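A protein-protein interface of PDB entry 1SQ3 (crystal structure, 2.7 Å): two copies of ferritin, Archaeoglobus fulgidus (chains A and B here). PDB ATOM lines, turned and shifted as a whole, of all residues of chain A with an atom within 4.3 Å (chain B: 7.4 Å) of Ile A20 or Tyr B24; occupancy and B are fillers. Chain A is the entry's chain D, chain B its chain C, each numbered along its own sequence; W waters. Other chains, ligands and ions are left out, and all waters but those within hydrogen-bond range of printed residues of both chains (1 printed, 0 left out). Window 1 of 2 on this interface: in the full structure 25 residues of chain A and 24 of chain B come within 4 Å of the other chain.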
ATOM      1  N   ILE A  16       3.724  -0.120   0.783  1.00  0.00           N
ATOM      2  CA  ILE A  16       3.141  -1.357   0.278  1.00  0.00           C
ATOM      3  C   ILE A  16       2.499  -2.112   1.430  1.00  0.00           C
ATOM      4  O   ILE A  16       1.332  -2.532   1.348  1.00  0.00           O
ATOM      5  CB  ILE A  16       4.203  -2.258  -0.403  1.00  0.00           C
ATOM      6  CG1 ILE A  16       4.526  -1.759  -1.813  1.00  0.00           C
ATOM      7  CG2 ILE A  16       3.701  -3.676  -0.485  1.00  0.00           C
ATOM      8  CD1 ILE A  16       5.877  -2.178  -2.290  1.00  0.00           C
ATOM      9  N   ASN A  17       3.243  -2.274   2.521  1.00  0.00           N
ATOM     10  CA  ASN A  17       2.645  -2.813   3.751  1.00  0.00           C
ATOM     11  C   ASN A  17       1.388  -2.035   4.201  1.00  0.00           C
ATOM     12  O   ASN A  17       0.358  -2.630   4.487  1.00  0.00           O
ATOM     13  CB  ASN A  17       3.662  -2.884   4.883  1.00  0.00           C
ATOM     14  CG  ASN A  17       3.079  -3.504   6.137  1.00  0.00           C
ATOM     15  OD1 ASN A  17       3.035  -4.734   6.282  1.00  0.00           O
ATOM     16  ND2 ASN A  17       2.540  -2.654   7.014  1.00  0.00           N
ATOM     17  N   ALA A  18       1.425  -0.709   4.145  1.00  0.00           N
ATOM     18  CA  ALA A  18       0.243   0.058   4.506  1.00  0.00           C
ATOM     19  C   ALA A  18      -0.916  -0.156   3.520  1.00  0.00           C
ATOM     20  O   ALA A  18      -2.061  -0.111   3.917  1.00  0.00           O
ATOM     21  CB  ALA A  18       0.579   1.544   4.647  1.00  0.00           C
ATOM     22  N   GLU A  19      -0.665  -0.327   2.229  1.00  0.00           N
ATOM     23  CA  GLU A  19      -1.795  -0.546   1.325  1.00  0.00           C
ATOM     24  C   GLU A  19      -2.364  -1.911   1.654  1.00  0.00           C
ATOM     25  O   GLU A  19      -3.577  -2.074   1.713  1.00  0.00           O
ATOM     26  CB  GLU A  19      -1.412  -0.512  -0.152  1.00  0.00           C
ATOM     27  CG  GLU A  19      -1.006   0.850  -0.666  1.00  0.00           C
ATOM     28  CD  GLU A  19      -2.139   1.854  -0.744  1.00  0.00           C
ATOM     29  OE1 GLU A  19      -3.355   1.487  -1.066  1.00  0.00           O
ATOM     30  OE2 GLU A  19      -1.730   3.049  -0.569  1.00  0.00           O
ATOM     31  N   ILE A  20      -1.503  -2.894   1.913  1.00  0.00           N
ATOM     32  CA  ILE A  20      -2.018  -4.219   2.263  1.00  0.00           C
ATOM     33  C   ILE A  20      -2.761  -4.185   3.599  1.00  0.00           C
ATOM     34  O   ILE A  20      -3.814  -4.808   3.741  1.00  0.00           O
ATOM     35  CB  ILE A  20      -0.902  -5.280   2.310  1.00  0.00           C
ATOM     36  CG1 ILE A  20      -0.360  -5.511   0.907  1.00  0.00           C
ATOM     37  CG2 ILE A  20      -1.449  -6.603   2.843  1.00  0.00           C
ATOM     38  CD1 ILE A  20       0.878  -6.370   0.874  1.00  0.00           C
ATOM     39  N   TYR A  21      -2.246  -3.446   4.573  1.00  0.00           N
ATOM     40  CA  TYR A  21      -2.988  -3.292   5.823  1.00  0.00           C
ATOM     41  C   TYR A  21      -4.375  -2.691   5.570  1.00  0.00           C
ATOM     42  O   TYR A  21      -5.374  -3.133   6.136  1.00  0.00           O
ATOM     43  CB  TYR A  21      -2.234  -2.448   6.865  1.00  0.00           C
ATOM     44  CG  TYR A  21      -3.029  -2.274   8.132  1.00  0.00           C
ATOM     45  CD1 TYR A  21      -3.260  -3.351   8.971  1.00  0.00           C
ATOM     46  CD2 TYR A  21      -3.635  -1.055   8.440  1.00  0.00           C
ATOM     47  CE1 TYR A  21      -4.043  -3.213  10.124  1.00  0.00           C
ATOM     48  CE2 TYR A  21      -4.441  -0.909   9.566  1.00  0.00           C
ATOM     49  CZ  TYR A  21      -4.647  -1.997  10.401  1.00  0.00           C
ATOM     50  OH  TYR A  21      -5.432  -1.869  11.533  1.00  0.00           O
ATOM     51  N   SER A  22      -4.434  -1.651   4.758  1.00  0.00           N
ATOM     52  CA  SER A  22      -5.713  -1.037   4.457  1.00  0.00           C
ATOM     53  C   SER A  22      -6.684  -2.086   3.912  1.00  0.00           C
ATOM     54  O   SER A  22      -7.839  -2.164   4.312  1.00  0.00           O
ATOM     55  CB  SER A  22      -5.514   0.094   3.453  1.00  0.00           C
ATOM     56  OG  SER A  22      -4.647   1.059   4.024  1.00  0.00           O
ATOM     57  N   ALA A  23      -6.201  -2.933   3.026  1.00  0.00           N
ATOM     58  CA  ALA A  23      -7.067  -3.931   2.450  1.00  0.00           C
ATOM     59  C   ALA A  23      -7.591  -4.822   3.579  1.00  0.00           C
ATOM     60  O   ALA A  23      -8.785  -5.135   3.649  1.00  0.00           O
ATOM     61  CB  ALA A  23      -6.294  -4.742   1.430  1.00  0.00           C
ATOM     62  N   TYR A  24      -6.680  -5.191   4.473  1.00  0.00           N
ATOM     63  CA  TYR A  24      -6.978  -6.100   5.580  1.00  0.00           C
ATOM     64  C   TYR A  24      -7.949  -5.505   6.618  1.00  0.00           C
ATOM     65  O   TYR A  24      -8.798  -6.200   7.149  1.00  0.00           O
ATOM     66  CB  TYR A  24      -5.673  -6.492   6.275  1.00  0.00           C
ATOM     67  CG  TYR A  24      -5.666  -7.868   6.906  1.00  0.00           C
ATOM     68  CD1 TYR A  24      -6.042  -8.993   6.181  1.00  0.00           C
ATOM     69  CD2 TYR A  24      -5.168  -8.050   8.182  1.00  0.00           C
ATOM     70  CE1 TYR A  24      -6.009 -10.244   6.755  1.00  0.00           C
ATOM     71  CE2 TYR A  24      -5.122  -9.290   8.754  1.00  0.00           C
ATOM     72  CZ  TYR A  24      -5.522 -10.390   8.036  1.00  0.00           C
ATOM     73  OH  TYR A  24      -5.472 -11.631   8.635  1.00  0.00           O
ATOM     74  N   ALA A  56      -1.515  -2.005  -3.852  1.00  0.00           N
ATOM     75  CA  ALA A  56      -0.278  -2.500  -3.271  1.00  0.00           C
ATOM     76  C   ALA A  56       0.589  -3.086  -4.356  1.00  0.00           C
ATOM     77  O   ALA A  56       1.765  -2.741  -4.446  1.00  0.00           O
ATOM     78  CB  ALA A  56      -0.556  -3.524  -2.198  1.00  0.00           C
ATOM     79  N   LEU A  72       8.878  -7.603   2.266  1.00  0.00           N
ATOM     80  CA  LEU A  72       7.521  -7.682   2.812  1.00  0.00           C
ATOM     81  C   LEU A  72       7.602  -7.727   4.330  1.00  0.00           C
ATOM     82  O   LEU A  72       8.466  -8.412   4.867  1.00  0.00           O
ATOM     83  CB  LEU A  72       6.790  -8.930   2.306  1.00  0.00           C
ATOM     84  CG  LEU A  72       6.434  -8.961   0.815  1.00  0.00           C
ATOM     85  CD1 LEU A  72       5.942 -10.346   0.408  1.00  0.00           C
ATOM     86  CD2 LEU A  72       5.384  -7.900   0.505  1.00  0.00           C
ATOM     87  N   TYR A  73       6.716  -6.982   4.995  1.00  0.00           N
ATOM     88  CA  TYR A  73       6.642  -6.922   6.464  1.00  0.00           C
ATOM     89  C   TYR A  73       5.352  -7.518   7.007  1.00  0.00           C
ATOM     90  O   TYR A  73       4.363  -7.625   6.298  1.00  0.00           O
ATOM     91  CB  TYR A  73       6.698  -5.468   6.957  1.00  0.00           C
ATOM     92  CG  TYR A  73       7.946  -4.731   6.566  1.00  0.00           C
ATOM     93  CD1 TYR A  73       9.108  -4.844   7.321  1.00  0.00           C
ATOM     94  CD2 TYR A  73       7.991  -3.989   5.389  1.00  0.00           C
ATOM     95  CE1 TYR A  73      10.269  -4.202   6.942  1.00  0.00           C
ATOM     96  CE2 TYR A  73       9.144  -3.340   5.005  1.00  0.00           C
ATOM     97  CZ  TYR A  73      10.280  -3.455   5.788  1.00  0.00           C
ATOM     98  OH  TYR A  73      11.429  -2.832   5.397  1.00  0.00           O
ATOM     99  N   VAL A  75       1.773  -8.017   8.508  1.00  0.00           N
ATOM    100  CA  VAL A  75       0.566  -7.195   8.493  1.00  0.00           C
ATOM    101  C   VAL A  75      -0.124  -7.197   9.863  1.00  0.00           C
ATOM    102  O   VAL A  75      -0.540  -8.253  10.340  1.00  0.00           O
ATOM    103  CB  VAL A  75      -0.445  -7.681   7.437  1.00  0.00           C
ATOM    104  CG1 VAL A  75      -1.492  -6.633   7.190  1.00  0.00           C
ATOM    105  CG2 VAL A  75       0.235  -8.000   6.163  1.00  0.00           C
ATOM    106  N   ALA B  18      -3.757 -19.091   7.880  1.00  0.00           N
ATOM    107  CA  ALA B  18      -2.713 -19.905   7.260  1.00  0.00           C
ATOM    108  C   ALA B  18      -2.779 -19.823   5.742  1.00  0.00           C
ATOM    109  O   ALA B  18      -1.741 -19.826   5.078  1.00  0.00           O
ATOM    110  CB  ALA B  18      -2.791 -21.355   7.728  1.00  0.00           C
ATOM    111  N   GLU B  19      -3.975 -19.696   5.182  1.00  0.00           N
ATOM    112  CA  GLU B  19      -4.064 -19.593   3.718  1.00  0.00           C
ATOM    113  C   GLU B  19      -3.518 -18.238   3.259  1.00  0.00           C
ATOM    114  O   GLU B  19      -2.819 -18.149   2.243  1.00  0.00           O
ATOM    115  CB  GLU B  19      -5.479 -19.819   3.193  1.00  0.00           C
ATOM    116  CG  GLU B  19      -6.026 -21.223   3.427  1.00  0.00           C
ATOM    117  CD  GLU B  19      -5.498 -22.300   2.469  1.00  0.00           C
ATOM    118  OE1 GLU B  19      -4.996 -22.017   1.321  1.00  0.00           O
ATOM    119  OE2 GLU B  19      -5.702 -23.480   2.847  1.00  0.00           O
ATOM    120  N   ILE B  20      -3.782 -17.193   4.040  1.00  0.00           N
ATOM    121  CA  ILE B  20      -3.295 -15.862   3.668  1.00  0.00           C
ATOM    122  C   ILE B  20      -1.769 -15.766   3.812  1.00  0.00           C
ATOM    123  O   ILE B  20      -1.087 -15.186   2.964  1.00  0.00           O
ATOM    124  CB  ILE B  20      -3.994 -14.770   4.488  1.00  0.00           C
ATOM    125  CG1 ILE B  20      -5.465 -14.702   4.102  1.00  0.00           C
ATOM    126  CG2 ILE B  20      -3.355 -13.435   4.240  1.00  0.00           C
ATOM    127  CD1 ILE B  20      -6.306 -13.840   5.040  1.00  0.00           C
ATOM    128  N   TYR B  21      -1.212 -16.368   4.850  1.00  0.00           N
ATOM    129  CA  TYR B  21       0.239 -16.312   5.012  1.00  0.00           C
ATOM    130  C   TYR B  21       0.914 -17.083   3.872  1.00  0.00           C
ATOM    131  O   TYR B  21       1.941 -16.651   3.374  1.00  0.00           O
ATOM    132  CB  TYR B  21       0.692 -16.832   6.388  1.00  0.00           C
ATOM    133  CG  TYR B  21       2.193 -17.057   6.467  1.00  0.00           C
ATOM    134  CD1 TYR B  21       2.744 -18.262   6.038  1.00  0.00           C
ATOM    135  CD2 TYR B  21       3.063 -16.046   6.870  1.00  0.00           C
ATOM    136  CE1 TYR B  21       4.106 -18.464   6.015  1.00  0.00           C
ATOM    137  CE2 TYR B  21       4.446 -16.238   6.823  1.00  0.00           C
ATOM    138  CZ  TYR B  21       4.960 -17.452   6.387  1.00  0.00           C
ATOM    139  OH  TYR B  21       6.321 -17.707   6.346  1.00  0.00           O
ATOM    140  N   SER B  22       0.304 -18.177   3.412  1.00  0.00           N
ATOM    141  CA  SER B  22       0.815 -18.889   2.233  1.00  0.00           C
ATOM    142  C   SER B  22       0.806 -17.982   1.001  1.00  0.00           C
ATOM    143  O   SER B  22       1.748 -17.970   0.206  1.00  0.00           O
ATOM    144  CB  SER B  22      -0.003 -20.151   1.933  1.00  0.00           C
ATOM    145  OG  SER B  22      -0.153 -20.961   3.087  1.00  0.00           O
ATOM    146  N   ALA B  23      -0.269 -17.240   0.811  1.00  0.00           N
ATOM    147  CA  ALA B  23      -0.279 -16.282  -0.275  1.00  0.00           C
ATOM    148  C   ALA B  23       0.918 -15.363  -0.118  1.00  0.00           C
ATOM    149  O   ALA B  23       1.613 -15.050  -1.075  1.00  0.00           O
ATOM    150  CB  ALA B  23      -1.550 -15.477  -0.230  1.00  0.00           C
ATOM    151  N   TYR B  24       1.103 -14.870   1.094  1.00  0.00           N
ATOM    152  CA  TYR B  24       2.086 -13.853   1.344  1.00  0.00           C
ATOM    153  C   TYR B  24       3.479 -14.480   1.232  1.00  0.00           C
ATOM    154  O   TYR B  24       4.464 -13.797   0.920  1.00  0.00           O
ATOM    155  CB  TYR B  24       1.857 -13.312   2.742  1.00  0.00           C
ATOM    156  CG  TYR B  24       2.369 -11.929   3.008  1.00  0.00           C
ATOM    157  CD1 TYR B  24       2.130 -10.899   2.138  1.00  0.00           C
ATOM    158  CD2 TYR B  24       2.985 -11.639   4.200  1.00  0.00           C
ATOM    159  CE1 TYR B  24       2.556  -9.624   2.411  1.00  0.00           C
ATOM    160  CE2 TYR B  24       3.399 -10.363   4.499  1.00  0.00           C
ATOM    161  CZ  TYR B  24       3.191  -9.353   3.602  1.00  0.00           C
ATOM    162  OH  TYR B  24       3.628  -8.079   3.932  1.00  0.00           O
ATOM    163  N   LEU B  25       3.579 -15.779   1.498  1.00  0.00           N
ATOM    164  CA  LEU B  25       4.874 -16.440   1.415  1.00  0.00           C
ATOM    165  C   LEU B  25       5.206 -16.483  -0.063  1.00  0.00           C
ATOM    166  O   LEU B  25       6.304 -16.133  -0.481  1.00  0.00           O
ATOM    167  CB  LEU B  25       4.798 -17.854   1.992  1.00  0.00           C
ATOM    168  CG  LEU B  25       5.950 -18.824   1.677  1.00  0.00           C
ATOM    169  CD1 LEU B  25       7.309 -18.241   2.052  1.00  0.00           C
ATOM    170  CD2 LEU B  25       5.741 -20.172   2.379  1.00  0.00           C
ATOM    171  N   TYR B  26       4.207 -16.827  -0.863  1.00  0.00           N
ATOM    172  CA  TYR B  26       4.423 -16.986  -2.274  1.00  0.00           C
ATOM    173  C   TYR B  26       4.728 -15.616  -2.892  1.00  0.00           C
ATOM    174  O   TYR B  26       5.567 -15.513  -3.800  1.00  0.00           O
ATOM    175  CB  TYR B  26       3.230 -17.714  -2.919  1.00  0.00           C
ATOM    176  CG  TYR B  26       3.084 -19.148  -2.444  1.00  0.00           C
ATOM    177  CD1 TYR B  26       4.190 -19.877  -2.030  1.00  0.00           C
ATOM    178  CD2 TYR B  26       1.849 -19.751  -2.342  1.00  0.00           C
ATOM    179  CE1 TYR B  26       4.075 -21.158  -1.508  1.00  0.00           C
ATOM    180  CE2 TYR B  26       1.725 -21.051  -1.860  1.00  0.00           C
ATOM    181  CZ  TYR B  26       2.841 -21.747  -1.434  1.00  0.00           C
ATOM    182  OH  TYR B  26       2.737 -23.053  -0.994  1.00  0.00           O
ATOM    183  N   LEU B  27       4.177 -14.548  -2.315  1.00  0.00           N
ATOM    184  CA  LEU B  27       4.455 -13.214  -2.840  1.00  0.00           C
ATOM    185  C   LEU B  27       5.896 -12.830  -2.557  1.00  0.00           C
ATOM    186  O   LEU B  27       6.525 -12.141  -3.348  1.00  0.00           O
ATOM    187  CB  LEU B  27       3.513 -12.179  -2.242  1.00  0.00           C
ATOM    188  CG  LEU B  27       3.688 -10.746  -2.744  1.00  0.00           C
ATOM    189  CD1 LEU B  27       3.244 -10.578  -4.187  1.00  0.00           C
ATOM    190  CD2 LEU B  27       2.876  -9.835  -1.864  1.00  0.00           C
ATOM    191  N   SER B  28       6.413 -13.261  -1.411  1.00  0.00           N
ATOM    192  CA  SER B  28       7.814 -13.018  -1.088  1.00  0.00           C
ATOM    193  C   SER B  28       8.730 -13.751  -2.051  1.00  0.00           C
ATOM    194  O   SER B  28       9.718 -13.193  -2.495  1.00  0.00           O
ATOM    195  CB  SER B  28       8.150 -13.452   0.333  1.00  0.00           C
ATOM    196  OG  SER B  28       9.493 -13.098   0.629  1.00  0.00           O
ATOM    197  N   MET B  29       8.420 -15.007  -2.341  1.00  0.00           N
ATOM    198  CA  MET B  29       9.095 -15.740  -3.405  1.00  0.00           C
ATOM    199  C   MET B  29       9.008 -15.054  -4.786  1.00  0.00           C
ATOM    200  O   MET B  29       9.979 -15.030  -5.533  1.00  0.00           O
ATOM    201  CB  MET B  29       8.511 -17.157  -3.496  1.00  0.00           C
ATOM    202  CG  MET B  29       9.067 -18.129  -2.458  1.00  0.00           C
ATOM    203  SD  MET B  29       8.204 -19.856  -2.553  1.00  0.00           S
ATOM    204  CE  MET B  29       9.090 -20.687  -1.033  1.00  0.00           C
ATOM    205  N   ALA B  30       7.856 -14.489  -5.125  1.00  0.00           N
ATOM    206  CA  ALA B  30       7.756 -13.689  -6.341  1.00  0.00           C
ATOM    207  C   ALA B  30       8.828 -12.597  -6.371  1.00  0.00           C
ATOM    208  O   ALA B  30       9.520 -12.420  -7.378  1.00  0.00           O
ATOM    209  CB  ALA B  30       6.369 -13.076  -6.472  1.00  0.00           C
ATOM    210  N   GLN B  48       0.047 -18.144  -7.739  1.00  0.00           N
ATOM    211  CA  GLN B  48      -0.191 -18.887  -6.507  1.00  0.00           C
ATOM    212  C   GLN B  48      -0.647 -17.966  -5.385  1.00  0.00           C
ATOM    213  O   GLN B  48      -1.558 -18.314  -4.633  1.00  0.00           O
ATOM    214  CB  GLN B  48       1.026 -19.699  -6.089  1.00  0.00           C
ATOM    215  CG  GLN B  48       0.685 -20.947  -5.287  1.00  0.00           C
ATOM    216  CD  GLN B  48      -0.346 -21.850  -5.958  1.00  0.00           C
ATOM    217  OE1 GLN B  48      -0.195 -22.210  -7.121  1.00  0.00           O
ATOM    218  NE2 GLN B  48      -1.317 -22.313  -5.200  1.00  0.00           N
ATOM    219  N   TRP B  49      -0.091 -16.756  -5.322  1.00  0.00           N
ATOM    220  CA  TRP B  49      -0.522 -15.781  -4.290  1.00  0.00           C
ATOM    221  C   TRP B  49      -2.010 -15.495  -4.431  1.00  0.00           C
ATOM    222  O   TRP B  49      -2.761 -15.662  -3.493  1.00  0.00           O
ATOM    223  CB  TRP B  49       0.386 -14.519  -4.257  1.00  0.00           C
ATOM    224  CG  TRP B  49      -0.238 -13.123  -4.256  1.00  0.00           C
ATOM    225  CD1 TRP B  49      -0.493 -12.345  -5.358  1.00  0.00           C
ATOM    226  CD2 TRP B  49      -0.459 -12.258  -3.118  1.00  0.00           C
ATOM    227  NE1 TRP B  49      -0.933 -11.101  -4.974  1.00  0.00           N
ATOM    228  CE2 TRP B  49      -0.935 -11.029  -3.608  1.00  0.00           C
ATOM    229  CE3 TRP B  49      -0.427 -12.442  -1.740  1.00  0.00           C
ATOM    230  CZ2 TRP B  49      -1.297  -9.986  -2.775  1.00  0.00           C
ATOM    231  CZ3 TRP B  49      -0.759 -11.391  -0.919  1.00  0.00           C
ATOM    232  CH2 TRP B  49      -1.212 -10.194  -1.435  1.00  0.00           C
ATOM    233  N   GLU B  52      -4.028 -18.649  -3.416  1.00  0.00           N
ATOM    234  CA  GLU B  52      -4.172 -18.883  -1.979  1.00  0.00           C
ATOM    235  C   GLU B  52      -5.131 -17.868  -1.327  1.00  0.00           C
ATOM    236  O   GLU B  52      -5.942 -18.222  -0.460  1.00  0.00           O
ATOM    237  CB  GLU B  52      -2.817 -18.926  -1.264  1.00  0.00           C
ATOM    238  CG  GLU B  52      -1.885 -20.044  -1.755  1.00  0.00           C
ATOM    239  CD  GLU B  52      -2.284 -21.468  -1.334  1.00  0.00           C
ATOM    240  OE1 GLU B  52      -3.302 -21.661  -0.605  1.00  0.00           O
ATOM    241  OE2 GLU B  52      -1.547 -22.431  -1.687  1.00  0.00           O
ATOM    242  N   LEU B  53      -5.108 -16.623  -1.808  1.00  0.00           N
ATOM    243  CA  LEU B  53      -6.078 -15.624  -1.357  1.00  0.00           C
ATOM    244  C   LEU B  53      -7.487 -16.107  -1.646  1.00  0.00           C
ATOM    245  O   LEU B  53      -8.379 -15.963  -0.829  1.00  0.00           O
ATOM    246  CB  LEU B  53      -5.851 -14.287  -2.044  1.00  0.00           C
ATOM    247  CG  LEU B  53      -5.125 -13.179  -1.278  1.00  0.00           C
ATOM    248  CD1 LEU B  53      -4.347 -13.678  -0.099  1.00  0.00           C
ATOM    249  CD2 LEU B  53      -4.217 -12.382  -2.184  1.00  0.00           C
ATOM    250  N   VAL B  75      -0.714 -11.218   9.939  1.00  0.00           N
ATOM    251  CA  VAL B  75       0.036 -11.980   8.976  1.00  0.00           C
ATOM    252  C   VAL B  75       1.526 -11.773   9.247  1.00  0.00           C
ATOM    253  O   VAL B  75       2.050 -10.655   9.140  1.00  0.00           O
ATOM    254  CB  VAL B  75      -0.296 -11.559   7.547  1.00  0.00           C
ATOM    255  CG1 VAL B  75       0.313 -12.538   6.576  1.00  0.00           C
ATOM    256  CG2 VAL B  75      -1.783 -11.493   7.345  1.00  0.00           C
ATOM    257  N   GLU B  76       2.184 -12.869   9.612  1.00  0.00           N
ATOM    258  CA  GLU B  76       3.602 -12.876   9.939  1.00  0.00           C
ATOM    259  C   GLU B  76       4.451 -12.386   8.772  1.00  0.00           C
ATOM    260  O   GLU B  76       4.086 -12.591   7.617  1.00  0.00           O
ATOM    261  CB  GLU B  76       4.031 -14.296  10.319  1.00  0.00           C
ATOM    262  CG  GLU B  76       4.099 -14.540  11.815  1.00  0.00           C
ATOM    263  CD  GLU B  76       5.328 -13.901  12.462  1.00  0.00           C
ATOM    264  OE1 GLU B  76       6.097 -13.132  11.812  1.00  0.00           O
ATOM    265  OE2 GLU B  76       5.512 -14.160  13.667  1.00  0.00           O
ATOM    266  N   GLU B  77       5.563 -11.717   9.082  1.00  0.00           N
ATOM    267  CA  GLU B  77       6.608 -11.434   8.102  1.00  0.00           C
ATOM    268  C   GLU B  77       7.244 -12.715   7.553  1.00  0.00           C
ATOM    269  O   GLU B  77       7.927 -13.430   8.277  1.00  0.00           O
ATOM    270  CB  GLU B  77       7.702 -10.546   8.701  1.00  0.00           C
ATOM    271  CG  GLU B  77       8.946 -10.495   7.830  1.00  0.00           C
ATOM    272  CD  GLU B  77      10.030  -9.566   8.345  1.00  0.00           C
ATOM    273  OE1 GLU B  77       9.726  -8.569   9.028  1.00  0.00           O
ATOM    274  OE2 GLU B  77      11.200  -9.781   7.974  1.00  0.00           O
ATOM    275  N   PRO B  78       7.081 -12.967   6.260  1.00  0.00           N
ATOM    276  CA  PRO B  78       7.567 -14.212   5.662  1.00  0.00           C
ATOM    277  C   PRO B  78       9.058 -14.110   5.486  1.00  0.00           C
ATOM    278  O   PRO B  78       9.561 -12.989   5.390  1.00  0.00           O
ATOM    279  CB  PRO B  78       6.907 -14.211   4.283  1.00  0.00           C
ATOM    280  CG  PRO B  78       6.824 -12.743   3.922  1.00  0.00           C
ATOM    281  CD  PRO B  78       6.575 -12.026   5.244  1.00  0.00           C
ATOM    282  N   PRO B  79       9.724 -15.232   5.263  1.00  0.00           N
ATOM    283  CA  PRO B  79      11.140 -15.210   4.861  1.00  0.00           C
ATOM    284  C   PRO B  79      11.288 -14.620   3.460  1.00  0.00           C
ATOM    285  O   PRO B  79      10.304 -14.571   2.720  1.00  0.00           O
ATOM    286  CB  PRO B  79      11.546 -16.689   4.876  1.00  0.00           C
ATOM    287  CG  PRO B  79      10.259 -17.461   4.732  1.00  0.00           C
ATOM    288  CD  PRO B  79       9.157 -16.590   5.306  1.00  0.00           C
ATOM    289  N   TRP B  82      15.981 -17.467  -0.597  1.00  0.00           N
ATOM    290  CA  TRP B  82      16.296 -18.881  -0.753  1.00  0.00           C
ATOM    291  C   TRP B  82      17.600 -19.045  -1.521  1.00  0.00           C
ATOM    292  O   TRP B  82      18.033 -18.151  -2.281  1.00  0.00           O
ATOM    293  CB  TRP B  82      15.184 -19.619  -1.515  1.00  0.00           C
ATOM    294  CG  TRP B  82      13.915 -19.661  -0.752  1.00  0.00           C
ATOM    295  CD1 TRP B  82      13.452 -20.685   0.017  1.00  0.00           C
ATOM    296  CD2 TRP B  82      12.982 -18.591  -0.607  1.00  0.00           C
ATOM    297  NE1 TRP B  82      12.287 -20.308   0.640  1.00  0.00           N
ATOM    298  CE2 TRP B  82      11.994 -19.015   0.295  1.00  0.00           C
ATOM    299  CE3 TRP B  82      12.890 -17.302  -1.140  1.00  0.00           C
ATOM    300  CZ2 TRP B  82      10.910 -18.227   0.630  1.00  0.00           C
ATOM    301  CZ3 TRP B  82      11.834 -16.505  -0.769  1.00  0.00           C
ATOM    302  CH2 TRP B  82      10.851 -16.972   0.093  1.00  0.00           C
HETATM  303  O   HOH W   1       4.754  -5.487   3.591  1.00  0.00           O
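The side-chain hydroxyl of Tyr B24 is in hydrogen-bond range of the backbone carbonyl oxygen of Tyr A73.
O of Val B75 sits at hydrogen-bond distance from N of Val A75 (2.7 Å).
The backbone carbonyl oxygen of Pro B79 sits at hydrogen-bond distance from the side-chain hydroxyl of Ser B28 (2.7 Å).
The side-chain amide oxygen (OD1) of Asn A17 lies close to the backbone carbonyl oxygen (O) of Tyr A73 (3.2 Å).
Among the printed residues, pairs that only touch across the chains: Ile A20 with Tyr B24 (3.97 Å), Tyr A24 with Ile B20 (3.995 Å), Tyr A24 with Val B75 (3.9 Å), Leu A72 with Tyr B24 (3.7 Å), Leu A72 with Leu B27 (3.9 Å), Leu A72 with Ser B28 (3.5 Å) and Leu A72 with Glu B77 (3.7 Å).
Ile A20 touches one residue of chain B.
Of the printed residues of chain B, Leu A72 touches Tyr B24 (3.7 Å), Leu B27 (3.9 Å), Ser B28 (3.5 Å) and Glu B77 (3.7 Å).
Printed residues of chain B within 4 Å of Tyr A73: Tyr B24.
Of chain A, only Ile A20 (3.97 Å), Leu A72 (3.7 Å) and Tyr A73 (2.5 Å) come within 4 Å of Tyr B24.
Printed residues of chain A within 4 Å of Leu B27: Leu A72 (3.9 Å).
The nearest residue of chain A that does not touch Tyr B24 is Val A75 (4.1 Å).
The nearest printed residue of chain B that does not touch Val A75 is Tyr B24 (4.1 Å).
Of the 23 printed residues of chain B, 6 touch a printed residue of chain A.
Hydrophobic or aromatic side chains of chain B that line the printed part of chain A: Ile B20, Tyr B24, Leu B27 and Val B75.
Of the 13 printed residues of chain A, 5 touch a printed residue of chain B.
Printed residues of chain A that touch a printed residue of chain B: Ile A20, Tyr A24, Leu A72, Tyr A73 and Val A75.
Hydrophobic or aromatic side chains of chain A within 4 Å of the printed part of chain B: Ile A20, Tyr A24, Leu A72 and Val A75.
Among the printed residues, 9 pairs touch across the chains.
Ile A20 touches Tyr B24, and with the chains exchanged Tyr A24 touches Ile B20.
Tyr A24 touches Val B75, but with the chains exchanged Val A75 does not touch Tyr B24 (4.1 Å).
Val A75 touches its own counterpart, Val B75.
8 positions are printed for both chains.
Of the 9 pairs that touch across the chains among the printed residues, 3 have their exchanged pair printed and touching as well.
Water W1 lies within hydrogen-bond range of N of Tyr A73 (2.8 Å), OH of Tyr B24 (2.8 Å) and OD1 of Asn A17 (3.3 Å).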
